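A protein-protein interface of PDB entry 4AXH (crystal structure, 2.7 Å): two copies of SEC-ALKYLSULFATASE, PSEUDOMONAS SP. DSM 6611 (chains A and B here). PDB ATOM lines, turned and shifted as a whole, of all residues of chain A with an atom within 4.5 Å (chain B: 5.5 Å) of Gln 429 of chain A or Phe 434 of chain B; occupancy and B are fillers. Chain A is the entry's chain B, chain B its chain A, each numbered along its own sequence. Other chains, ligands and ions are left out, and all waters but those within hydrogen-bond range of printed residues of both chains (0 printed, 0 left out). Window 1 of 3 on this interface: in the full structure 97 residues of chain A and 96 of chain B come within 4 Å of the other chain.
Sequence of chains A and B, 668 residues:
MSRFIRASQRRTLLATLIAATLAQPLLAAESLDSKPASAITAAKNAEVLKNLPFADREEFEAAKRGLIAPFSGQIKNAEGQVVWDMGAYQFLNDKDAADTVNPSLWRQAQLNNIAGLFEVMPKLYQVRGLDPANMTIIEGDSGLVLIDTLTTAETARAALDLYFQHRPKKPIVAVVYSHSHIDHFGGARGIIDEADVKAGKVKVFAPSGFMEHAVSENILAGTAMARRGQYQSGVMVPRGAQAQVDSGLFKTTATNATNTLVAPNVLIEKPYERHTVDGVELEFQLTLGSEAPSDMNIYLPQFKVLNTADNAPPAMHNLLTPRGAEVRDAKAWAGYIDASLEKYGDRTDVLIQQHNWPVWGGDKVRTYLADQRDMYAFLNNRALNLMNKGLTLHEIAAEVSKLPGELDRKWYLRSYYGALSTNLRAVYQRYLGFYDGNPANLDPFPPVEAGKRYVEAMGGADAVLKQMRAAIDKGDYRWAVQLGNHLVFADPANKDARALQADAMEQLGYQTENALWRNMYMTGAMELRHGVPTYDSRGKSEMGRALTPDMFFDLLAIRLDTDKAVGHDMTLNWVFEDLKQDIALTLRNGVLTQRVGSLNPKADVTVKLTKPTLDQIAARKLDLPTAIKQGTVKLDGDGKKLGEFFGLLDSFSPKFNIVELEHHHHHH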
ATOM      1  N   LEU A 320       3.665   4.371 -20.203  1.00  0.00           N
ATOM      2  CA  LEU A 320       4.381   5.641 -20.240  1.00  0.00           C
ATOM      3  C   LEU A 320       4.755   6.050 -18.815  1.00  0.00           C
ATOM      4  O   LEU A 320       3.908   6.589 -18.089  1.00  0.00           O
ATOM      5  CB  LEU A 320       3.589   6.757 -20.947  1.00  0.00           C
ATOM      6  CG  LEU A 320       4.376   8.081 -21.185  1.00  0.00           C
ATOM      7  CD1 LEU A 320       5.387   7.946 -22.342  1.00  0.00           C
ATOM      8  CD2 LEU A 320       3.435   9.233 -21.405  1.00  0.00           C
ATOM      9  N   VAL A 327       7.250   5.223 -25.202  1.00  0.00           N
ATOM     10  CA  VAL A 327       6.061   4.378 -24.940  1.00  0.00           C
ATOM     11  C   VAL A 327       6.393   2.926 -25.141  1.00  0.00           C
ATOM     12  O   VAL A 327       7.229   2.579 -25.983  1.00  0.00           O
ATOM     13  CB  VAL A 327       4.815   4.686 -25.788  1.00  0.00           C
ATOM     14  CG1 VAL A 327       3.773   5.452 -24.978  1.00  0.00           C
ATOM     15  CG2 VAL A 327       5.176   5.346 -27.110  1.00  0.00           C
ATOM     16  N   LEU A 393      -7.613  10.772 -26.881  1.00  0.00           N
ATOM     17  CA  LEU A 393      -6.896  10.324 -25.685  1.00  0.00           C
ATOM     18  C   LEU A 393      -7.580  10.514 -24.336  1.00  0.00           C
ATOM     19  O   LEU A 393      -7.661   9.559 -23.560  1.00  0.00           O
ATOM     20  CB  LEU A 393      -5.427  10.797 -25.674  1.00  0.00           C
ATOM     21  CG  LEU A 393      -5.070  12.222 -25.244  1.00  0.00           C
ATOM     22  CD1 LEU A 393      -3.671  12.247 -24.685  1.00  0.00           C
ATOM     23  CD2 LEU A 393      -5.235  13.230 -26.376  1.00  0.00           C
ATOM     24  N   THR A 422      -3.725   6.881 -17.645  1.00  0.00           N
ATOM     25  CA  THR A 422      -2.430   7.190 -18.243  1.00  0.00           C
ATOM     26  C   THR A 422      -2.101   6.219 -19.382  1.00  0.00           C
ATOM     27  O   THR A 422      -1.728   6.658 -20.473  1.00  0.00           O
ATOM     28  CB  THR A 422      -1.355   7.176 -17.162  1.00  0.00           C
ATOM     29  OG1 THR A 422      -1.751   8.030 -16.095  1.00  0.00           O
ATOM     30  CG2 THR A 422       0.000   7.607 -17.689  1.00  0.00           C
ATOM     31  N   ARG A 425      -4.288   6.601 -22.469  1.00  0.00           N
ATOM     32  CA  ARG A 425      -3.783   7.796 -23.138  1.00  0.00           C
ATOM     33  C   ARG A 425      -2.478   7.436 -23.868  1.00  0.00           C
ATOM     34  O   ARG A 425      -2.323   7.787 -25.026  1.00  0.00           O
ATOM     35  CB  ARG A 425      -3.629   8.959 -22.134  1.00  0.00           C
ATOM     36  CG  ARG A 425      -4.991   9.495 -21.653  1.00  0.00           C
ATOM     37  CD  ARG A 425      -4.952  10.788 -20.861  1.00  0.00           C
ATOM     38  NE  ARG A 425      -4.845  10.534 -19.426  1.00  0.00           N
ATOM     39  CZ  ARG A 425      -5.711  10.940 -18.501  1.00  0.00           C
ATOM     40  NH1 ARG A 425      -6.767  11.669 -18.841  1.00  0.00           N
ATOM     41  NH2 ARG A 425      -5.509  10.647 -17.225  1.00  0.00           N
ATOM     42  N   ALA A 426      -1.621   6.626 -23.238  1.00  0.00           N
ATOM     43  CA  ALA A 426      -0.355   6.164 -23.799  1.00  0.00           C
ATOM     44  C   ALA A 426      -0.504   5.340 -25.081  1.00  0.00           C
ATOM     45  O   ALA A 426       0.316   5.510 -26.006  1.00  0.00           O
ATOM     46  CB  ALA A 426       0.417   5.380 -22.764  1.00  0.00           C
ATOM     47  N   VAL A 427      -1.534   4.434 -25.142  1.00  0.00           N
ATOM     48  CA  VAL A 427      -1.827   3.589 -26.337  1.00  0.00           C
ATOM     49  C   VAL A 427      -2.221   4.552 -27.498  1.00  0.00           C
ATOM     50  O   VAL A 427      -1.790   4.348 -28.632  1.00  0.00           O
ATOM     51  CB  VAL A 427      -2.881   2.432 -26.086  1.00  0.00           C
ATOM     52  CG1 VAL A 427      -3.082   1.555 -27.326  1.00  0.00           C
ATOM     53  CG2 VAL A 427      -2.489   1.548 -24.906  1.00  0.00           C
ATOM     54  N   TYR A 428      -2.962   5.627 -27.179  1.00  0.00           N
ATOM     55  CA  TYR A 428      -3.334   6.668 -28.125  1.00  0.00           C
ATOM     56  C   TYR A 428      -2.075   7.348 -28.652  1.00  0.00           C
ATOM     57  O   TYR A 428      -1.938   7.462 -29.860  1.00  0.00           O
ATOM     58  CB  TYR A 428      -4.274   7.708 -27.482  1.00  0.00           C
ATOM     59  CG  TYR A 428      -4.852   8.697 -28.466  1.00  0.00           C
ATOM     60  CD1 TYR A 428      -4.134   9.829 -28.859  1.00  0.00           C
ATOM     61  CD2 TYR A 428      -6.116   8.505 -29.010  1.00  0.00           C
ATOM     62  CE1 TYR A 428      -4.674  10.754 -29.753  1.00  0.00           C
ATOM     63  CE2 TYR A 428      -6.660   9.411 -29.915  1.00  0.00           C
ATOM     64  CZ  TYR A 428      -5.942  10.539 -30.276  1.00  0.00           C
ATOM     65  OH  TYR A 428      -6.499  11.408 -31.180  1.00  0.00           O
ATOM     66  N   GLN A 429      -1.160   7.794 -27.751  1.00  0.00           N
ATOM     67  CA  GLN A 429       0.133   8.406 -28.084  1.00  0.00           C
ATOM     68  C   GLN A 429       0.955   7.474 -28.990  1.00  0.00           C
ATOM     69  O   GLN A 429       1.447   7.899 -30.059  1.00  0.00           O
ATOM     70  CB  GLN A 429       0.930   8.751 -26.797  1.00  0.00           C
ATOM     71  CG  GLN A 429       2.411   9.118 -27.057  1.00  0.00           C
ATOM     72  CD  GLN A 429       3.262   9.228 -25.849  1.00  0.00           C
ATOM     73  OE1 GLN A 429       2.887   9.840 -24.856  1.00  0.00           O
ATOM     74  NE2 GLN A 429       4.463   8.677 -25.924  1.00  0.00           N
ATOM     75  N   ARG A 430       1.111   6.212 -28.555  1.00  0.00           N
ATOM     76  CA  ARG A 430       1.874   5.241 -29.319  1.00  0.00           C
ATOM     77  C   ARG A 430       1.391   5.028 -30.784  1.00  0.00           C
ATOM     78  O   ARG A 430       2.217   5.028 -31.697  1.00  0.00           O
ATOM     79  CB  ARG A 430       2.073   3.933 -28.517  1.00  0.00           C
ATOM     80  CG  ARG A 430       1.953   2.672 -29.335  1.00  0.00           C
ATOM     81  CD  ARG A 430       3.092   1.722 -29.212  1.00  0.00           C
ATOM     82  NE  ARG A 430       2.866   0.657 -30.190  1.00  0.00           N
ATOM     83  CZ  ARG A 430       3.820  -0.046 -30.773  1.00  0.00           C
ATOM     84  NH1 ARG A 430       5.094   0.169 -30.465  1.00  0.00           N
ATOM     85  NH2 ARG A 430       3.514  -0.961 -31.677  1.00  0.00           N
ATOM     86  N   TYR A 431       0.071   4.914 -31.009  1.00  0.00           N
ATOM     87  CA  TYR A 431      -0.487   4.643 -32.344  1.00  0.00           C
ATOM     88  C   TYR A 431      -0.840   5.874 -33.122  1.00  0.00           C
ATOM     89  O   TYR A 431      -0.859   5.815 -34.346  1.00  0.00           O
ATOM     90  CB  TYR A 431      -1.740   3.726 -32.259  1.00  0.00           C
ATOM     91  CG  TYR A 431      -1.443   2.285 -31.947  1.00  0.00           C
ATOM     92  CD1 TYR A 431      -0.988   1.417 -32.936  1.00  0.00           C
ATOM     93  CD2 TYR A 431      -1.620   1.780 -30.661  1.00  0.00           C
ATOM     94  CE1 TYR A 431      -0.663   0.099 -32.644  1.00  0.00           C
ATOM     95  CE2 TYR A 431      -1.347   0.443 -30.368  1.00  0.00           C
ATOM     96  CZ  TYR A 431      -0.875  -0.390 -31.365  1.00  0.00           C
ATOM     97  OH  TYR A 431      -0.580  -1.689 -31.095  1.00  0.00           O
ATOM     98  N   LEU A 432      -1.173   6.976 -32.437  1.00  0.00           N
ATOM     99  CA  LEU A 432      -1.574   8.212 -33.111  1.00  0.00           C
ATOM    100  C   LEU A 432      -0.715   9.416 -32.757  1.00  0.00           C
ATOM    101  O   LEU A 432      -0.313  10.163 -33.652  1.00  0.00           O
ATOM    102  CB  LEU A 432      -3.100   8.477 -32.980  1.00  0.00           C
ATOM    103  CG  LEU A 432      -4.043   7.342 -33.480  1.00  0.00           C
ATOM    104  CD1 LEU A 432      -5.497   7.619 -33.143  1.00  0.00           C
ATOM    105  CD2 LEU A 432      -3.871   7.053 -34.976  1.00  0.00           C
ATOM    106  N   GLY A 433      -0.400   9.570 -31.477  1.00  0.00           N
ATOM    107  CA  GLY A 433       0.445  10.662 -31.009  1.00  0.00           C
ATOM    108  C   GLY A 433      -0.270  11.678 -30.159  1.00  0.00           C
ATOM    109  O   GLY A 433      -1.490  11.592 -29.982  1.00  0.00           O
ATOM    110  N   LEU B 320       6.068  12.819 -36.965  1.00  0.00           N
ATOM    111  CA  LEU B 320       4.731  12.395 -36.548  1.00  0.00           C
ATOM    112  C   LEU B 320       3.723  12.863 -37.588  1.00  0.00           C
ATOM    113  O   LEU B 320       3.312  14.034 -37.551  1.00  0.00           O
ATOM    114  CB  LEU B 320       4.345  12.920 -35.122  1.00  0.00           C
ATOM    115  CG  LEU B 320       3.014  12.396 -34.547  1.00  0.00           C
ATOM    116  CD1 LEU B 320       3.163  10.986 -34.026  1.00  0.00           C
ATOM    117  CD2 LEU B 320       2.500  13.275 -33.439  1.00  0.00           C
ATOM    118  N   ALA B 325       0.302   8.159 -36.469  1.00  0.00           N
ATOM    119  CA  ALA B 325       1.309   7.089 -36.661  1.00  0.00           C
ATOM    120  C   ALA B 325       2.258   6.993 -35.470  1.00  0.00           C
ATOM    121  O   ALA B 325       2.222   7.832 -34.563  1.00  0.00           O
ATOM    122  CB  ALA B 325       2.118   7.345 -37.924  1.00  0.00           C
ATOM    123  N   LEU B 393       7.119  20.139 -24.047  1.00  0.00           N
ATOM    124  CA  LEU B 393       6.774  20.064 -25.473  1.00  0.00           C
ATOM    125  C   LEU B 393       6.357  21.343 -26.159  1.00  0.00           C
ATOM    126  O   LEU B 393       6.906  21.656 -27.217  1.00  0.00           O
ATOM    127  CB  LEU B 393       5.825  18.892 -25.788  1.00  0.00           C
ATOM    128  CG  LEU B 393       4.321  19.033 -25.559  1.00  0.00           C
ATOM    129  CD1 LEU B 393       3.571  18.110 -26.488  1.00  0.00           C
ATOM    130  CD2 LEU B 393       3.945  18.779 -24.117  1.00  0.00           C
ATOM    131  N   TYR B 428       9.880  15.257 -28.108  1.00  0.00           N
ATOM    132  CA  TYR B 428       9.473  15.256 -26.711  1.00  0.00           C
ATOM    133  C   TYR B 428       8.614  14.022 -26.448  1.00  0.00           C
ATOM    134  O   TYR B 428       8.928  13.303 -25.512  1.00  0.00           O
ATOM    135  CB  TYR B 428       8.720  16.535 -26.343  1.00  0.00           C
ATOM    136  CG  TYR B 428       8.449  16.683 -24.863  1.00  0.00           C
ATOM    137  CD1 TYR B 428       7.348  16.063 -24.264  1.00  0.00           C
ATOM    138  CD2 TYR B 428       9.281  17.455 -24.055  1.00  0.00           C
ATOM    139  CE1 TYR B 428       7.087  16.212 -22.900  1.00  0.00           C
ATOM    140  CE2 TYR B 428       9.031  17.605 -22.690  1.00  0.00           C
ATOM    141  CZ  TYR B 428       7.931  16.991 -22.121  1.00  0.00           C
ATOM    142  OH  TYR B 428       7.705  17.159 -20.777  1.00  0.00           O
ATOM    143  N   GLN B 429       7.563  13.767 -27.271  1.00  0.00           N
ATOM    144  CA  GLN B 429       6.690  12.580 -27.193  1.00  0.00           C
ATOM    145  C   GLN B 429       7.525  11.283 -27.272  1.00  0.00           C
ATOM    146  O   GLN B 429       7.381  10.402 -26.414  1.00  0.00           O
ATOM    147  CB  GLN B 429       5.626  12.601 -28.328  1.00  0.00           C
ATOM    148  CG  GLN B 429       4.883  11.259 -28.533  1.00  0.00           C
ATOM    149  CD  GLN B 429       4.073  11.171 -29.816  1.00  0.00           C
ATOM    150  OE1 GLN B 429       3.331  12.095 -30.177  1.00  0.00           O
ATOM    151  NE2 GLN B 429       4.141  10.026 -30.491  1.00  0.00           N
ATOM    152  N   ARG B 430       8.395  11.175 -28.305  1.00  0.00           N
ATOM    153  CA  ARG B 430       9.251  10.005 -28.497  1.00  0.00           C
ATOM    154  C   ARG B 430      10.148   9.666 -27.278  1.00  0.00           C
ATOM    155  O   ARG B 430      10.195   8.511 -26.887  1.00  0.00           O
ATOM    156  CB  ARG B 430      10.001  10.041 -29.854  1.00  0.00           C
ATOM    157  CG  ARG B 430      11.449   9.565 -29.824  1.00  0.00           C
ATOM    158  CD  ARG B 430      11.871   8.639 -30.952  1.00  0.00           C
ATOM    159  NE  ARG B 430      13.240   8.204 -30.678  1.00  0.00           N
ATOM    160  CZ  ARG B 430      13.736   6.998 -30.932  1.00  0.00           C
ATOM    161  NH1 ARG B 430      12.980   6.068 -31.495  1.00  0.00           N
ATOM    162  NH2 ARG B 430      14.992   6.707 -30.605  1.00  0.00           N
ATOM    163  N   LEU B 432      10.012  11.329 -24.041  1.00  0.00           N
ATOM    164  CA  LEU B 432       9.354  11.492 -22.735  1.00  0.00           C
ATOM    165  C   LEU B 432       7.846  11.121 -22.724  1.00  0.00           C
ATOM    166  O   LEU B 432       7.377  10.471 -21.779  1.00  0.00           O
ATOM    167  CB  LEU B 432       9.622  12.874 -22.111  1.00  0.00           C
ATOM    168  CG  LEU B 432      11.113  13.264 -21.910  1.00  0.00           C
ATOM    169  CD1 LEU B 432      11.257  14.697 -21.398  1.00  0.00           C
ATOM    170  CD2 LEU B 432      11.857  12.307 -20.986  1.00  0.00           C
ATOM    171  N   GLY B 433       7.120  11.520 -23.762  1.00  0.00           N
ATOM    172  CA  GLY B 433       5.699  11.222 -23.864  1.00  0.00           C
ATOM    173  C   GLY B 433       4.801  12.425 -23.742  1.00  0.00           C
ATOM    174  O   GLY B 433       5.280  13.534 -23.484  1.00  0.00           O
ATOM    175  N   PHE B 434       3.479  12.205 -23.921  1.00  0.00           N
ATOM    176  CA  PHE B 434       2.465  13.255 -23.934  1.00  0.00           C
ATOM    177  C   PHE B 434       2.413  14.066 -22.650  1.00  0.00           C
ATOM    178  O   PHE B 434       1.984  15.223 -22.682  1.00  0.00           O
ATOM    179  CB  PHE B 434       1.073  12.669 -24.275  1.00  0.00           C
ATOM    180  CG  PHE B 434       0.380  11.966 -23.121  1.00  0.00           C
ATOM    181  CD1 PHE B 434       0.607  10.616 -22.869  1.00  0.00           C
ATOM    182  CD2 PHE B 434      -0.462  12.672 -22.256  1.00  0.00           C
ATOM    183  CE1 PHE B 434       0.021   9.991 -21.770  1.00  0.00           C
ATOM    184  CE2 PHE B 434      -1.040  12.046 -21.149  1.00  0.00           C
ATOM    185  CZ  PHE B 434      -0.811  10.706 -20.929  1.00  0.00           C
ATOM    186  N   TYR B 435       2.757  13.439 -21.520  1.00  0.00           N
ATOM    187  CA  TYR B 435       2.671  14.055 -20.190  1.00  0.00           C
ATOM    188  C   TYR B 435       3.904  14.902 -19.898  1.00  0.00           C
ATOM    189  O   TYR B 435       5.026  14.394 -19.979  1.00  0.00           O
ATOM    190  CB  TYR B 435       2.447  12.955 -19.125  1.00  0.00           C
ATOM    191  CG  TYR B 435       2.539  13.423 -17.693  1.00  0.00           C
ATOM    192  CD1 TYR B 435       1.677  14.400 -17.201  1.00  0.00           C
ATOM    193  CD2 TYR B 435       3.456  12.854 -16.811  1.00  0.00           C
ATOM    194  CE1 TYR B 435       1.760  14.836 -15.880  1.00  0.00           C
ATOM    195  CE2 TYR B 435       3.518  13.253 -15.476  1.00  0.00           C
ATOM    196  CZ  TYR B 435       2.673  14.252 -15.018  1.00  0.00           C
ATOM    197  OH  TYR B 435       2.729  14.690 -13.724  1.00  0.00           O
ATOM    198  N   ASP B 436       3.691  16.186 -19.570  1.00  0.00           N
ATOM    199  CA  ASP B 436       4.775  17.157 -19.355  1.00  0.00           C
ATOM    200  C   ASP B 436       5.567  17.085 -18.042  1.00  0.00           C
ATOM    201  O   ASP B 436       6.614  17.731 -17.927  1.00  0.00           O
ATOM    202  CB  ASP B 436       4.328  18.597 -19.698  1.00  0.00           C
ATOM    203  CG  ASP B 436       3.293  19.235 -18.770  1.00  0.00           C
ATOM    204  OD1 ASP B 436       2.845  18.556 -17.817  1.00  0.00           O
ATOM    205  OD2 ASP B 436       2.944  20.428 -18.991  1.00  0.00           O
ATOM    206  N   ASN B 441      -1.459  18.530 -15.106  1.00  0.00           N
ATOM    207  CA  ASN B 441      -1.814  17.917 -16.382  1.00  0.00           C
ATOM    208  C   ASN B 441      -1.772  16.374 -16.316  1.00  0.00           C
ATOM    209  O   ASN B 441      -1.648  15.717 -17.363  1.00  0.00           O
ATOM    210  CB  ASN B 441      -0.898  18.436 -17.497  1.00  0.00           C
ATOM    211  CG  ASN B 441      -0.841  19.931 -17.603  1.00  0.00           C
ATOM    212  OD1 ASN B 441       0.165  20.554 -17.245  1.00  0.00           O
ATOM    213  ND2 ASN B 441      -1.915  20.547 -18.093  1.00  0.00           N
ATOM    214  N   LEU B 442      -1.875  15.794 -15.103  1.00  0.00           N
ATOM    215  CA  LEU B 442      -1.826  14.341 -14.942  1.00  0.00           C
ATOM    216  C   LEU B 442      -3.095  13.637 -15.448  1.00  0.00           C
ATOM    217  O   LEU B 442      -3.006  12.581 -16.078  1.00  0.00           O
ATOM    218  CB  LEU B 442      -1.514  13.980 -13.482  1.00  0.00           C
ATOM    219  CG  LEU B 442      -1.152  12.534 -13.134  1.00  0.00           C
ATOM    220  CD1 LEU B 442      -0.055  11.980 -14.012  1.00  0.00           C
ATOM    221  CD2 LEU B 442      -0.734  12.437 -11.707  1.00  0.00           C
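The backbone NH (N) of Ala 325 of chain B sits at hydrogen-bond distance from the backbone carbonyl oxygen (O) of Tyr 431 of chain A, at 3.4 Å. The backbone carbonyl oxygen (O) of Gln 429 of chain B is in hydrogen-bond range of the side-chain amide nitrogen (NE2) of Gln 429 of chain A. The backbone NH (N) of Phe 434 of chain B lies within hydrogen-bond range of the side-chain amide oxygen (OE1) of Gln 429 of chain A (2.6 Å). The backbone carbonyl oxygen (O) of Leu 442 of chain B sits at hydrogen-bond distance from the guanidinium group (NH2) of Arg 425 of chain A (3.4 Å).
N of Gly 433 of chain B sits at hydrogen-bond distance from O of Tyr 428 of chain B, at 3.1 Å. The backbone carbonyl oxygen of Tyr 428 of chain A sits at hydrogen-bond distance from the backbone NH of Gly 433 of chain A, at 3.1 Å.
Among the printed residues, merely in contact across the chains: Leu 320 of chain A with Leu 432 of chain B, Leu 320 of chain A with Gly 433 of chain B, Leu 320 of chain A with Phe 434 of chain B, Thr 422 of chain A with Phe 434 of chain B, Arg 425 of chain A with Phe 434 of chain B, Gln 429 of chain A with Gly 433 of chain B, Leu 432 of chain A with Leu 320 of chain B, Leu 432 of chain A with Ala 325 of chain B and Gly 433 of chain A with Gln 429 of chain B.
Gln 429 of chain A touches just these residues of chain B: Gln 429, Gly 433 and Phe 434. Printed residues of chain B within 4 Å of Gly 433 of chain A: Gln 429. Of the printed residues of chain A, Ala 325 of chain B touches Tyr 431 and Leu 432. Printed residues of chain A within 4 Å of Phe 434 of chain B: Leu 320 (3.5 Å), Thr 422 (3.98 Å), Arg 425 (3.5 Å) and Gln 429 (2.6 Å). The nearest residue of chain B that does not touch Gln 429 of chain A is Ala 325 of chain B (4.6 Å). The nearest printed residue of chain B that does not touch Thr 422 of chain A is Leu 442 of chain B (4.7 Å).
Printed residues of chain A that touch a printed residue of chain B: Leu 320, Thr 422, Arg 425, Gln 429, Tyr 431, Leu 432 and Gly 433. Hydrophobic or aromatic side chains of chain A within 4 Å of the printed part of chain B: Leu 320. Along chain A the printed residues that touch a printed residue of chain B span positions 320 to 433.
Leu 320 of chain A touches Leu 432 of chain B, and with the chains exchanged Leu 432 of chain A touches Leu 320 of chain B. Leu 320 of chain A touches Gly 433 of chain B, but with the chains exchanged Gly 433 of chain A does not touch Leu 320 of chain B (4.1 Å). Gln 429 of chain B touches its own counterpart, Gln 429 of chain A. Gln 429 of chain A touches Gly 433 of chain B, and with the chains exchanged Gly 433 of chain A touches Gln 429 of chain B.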
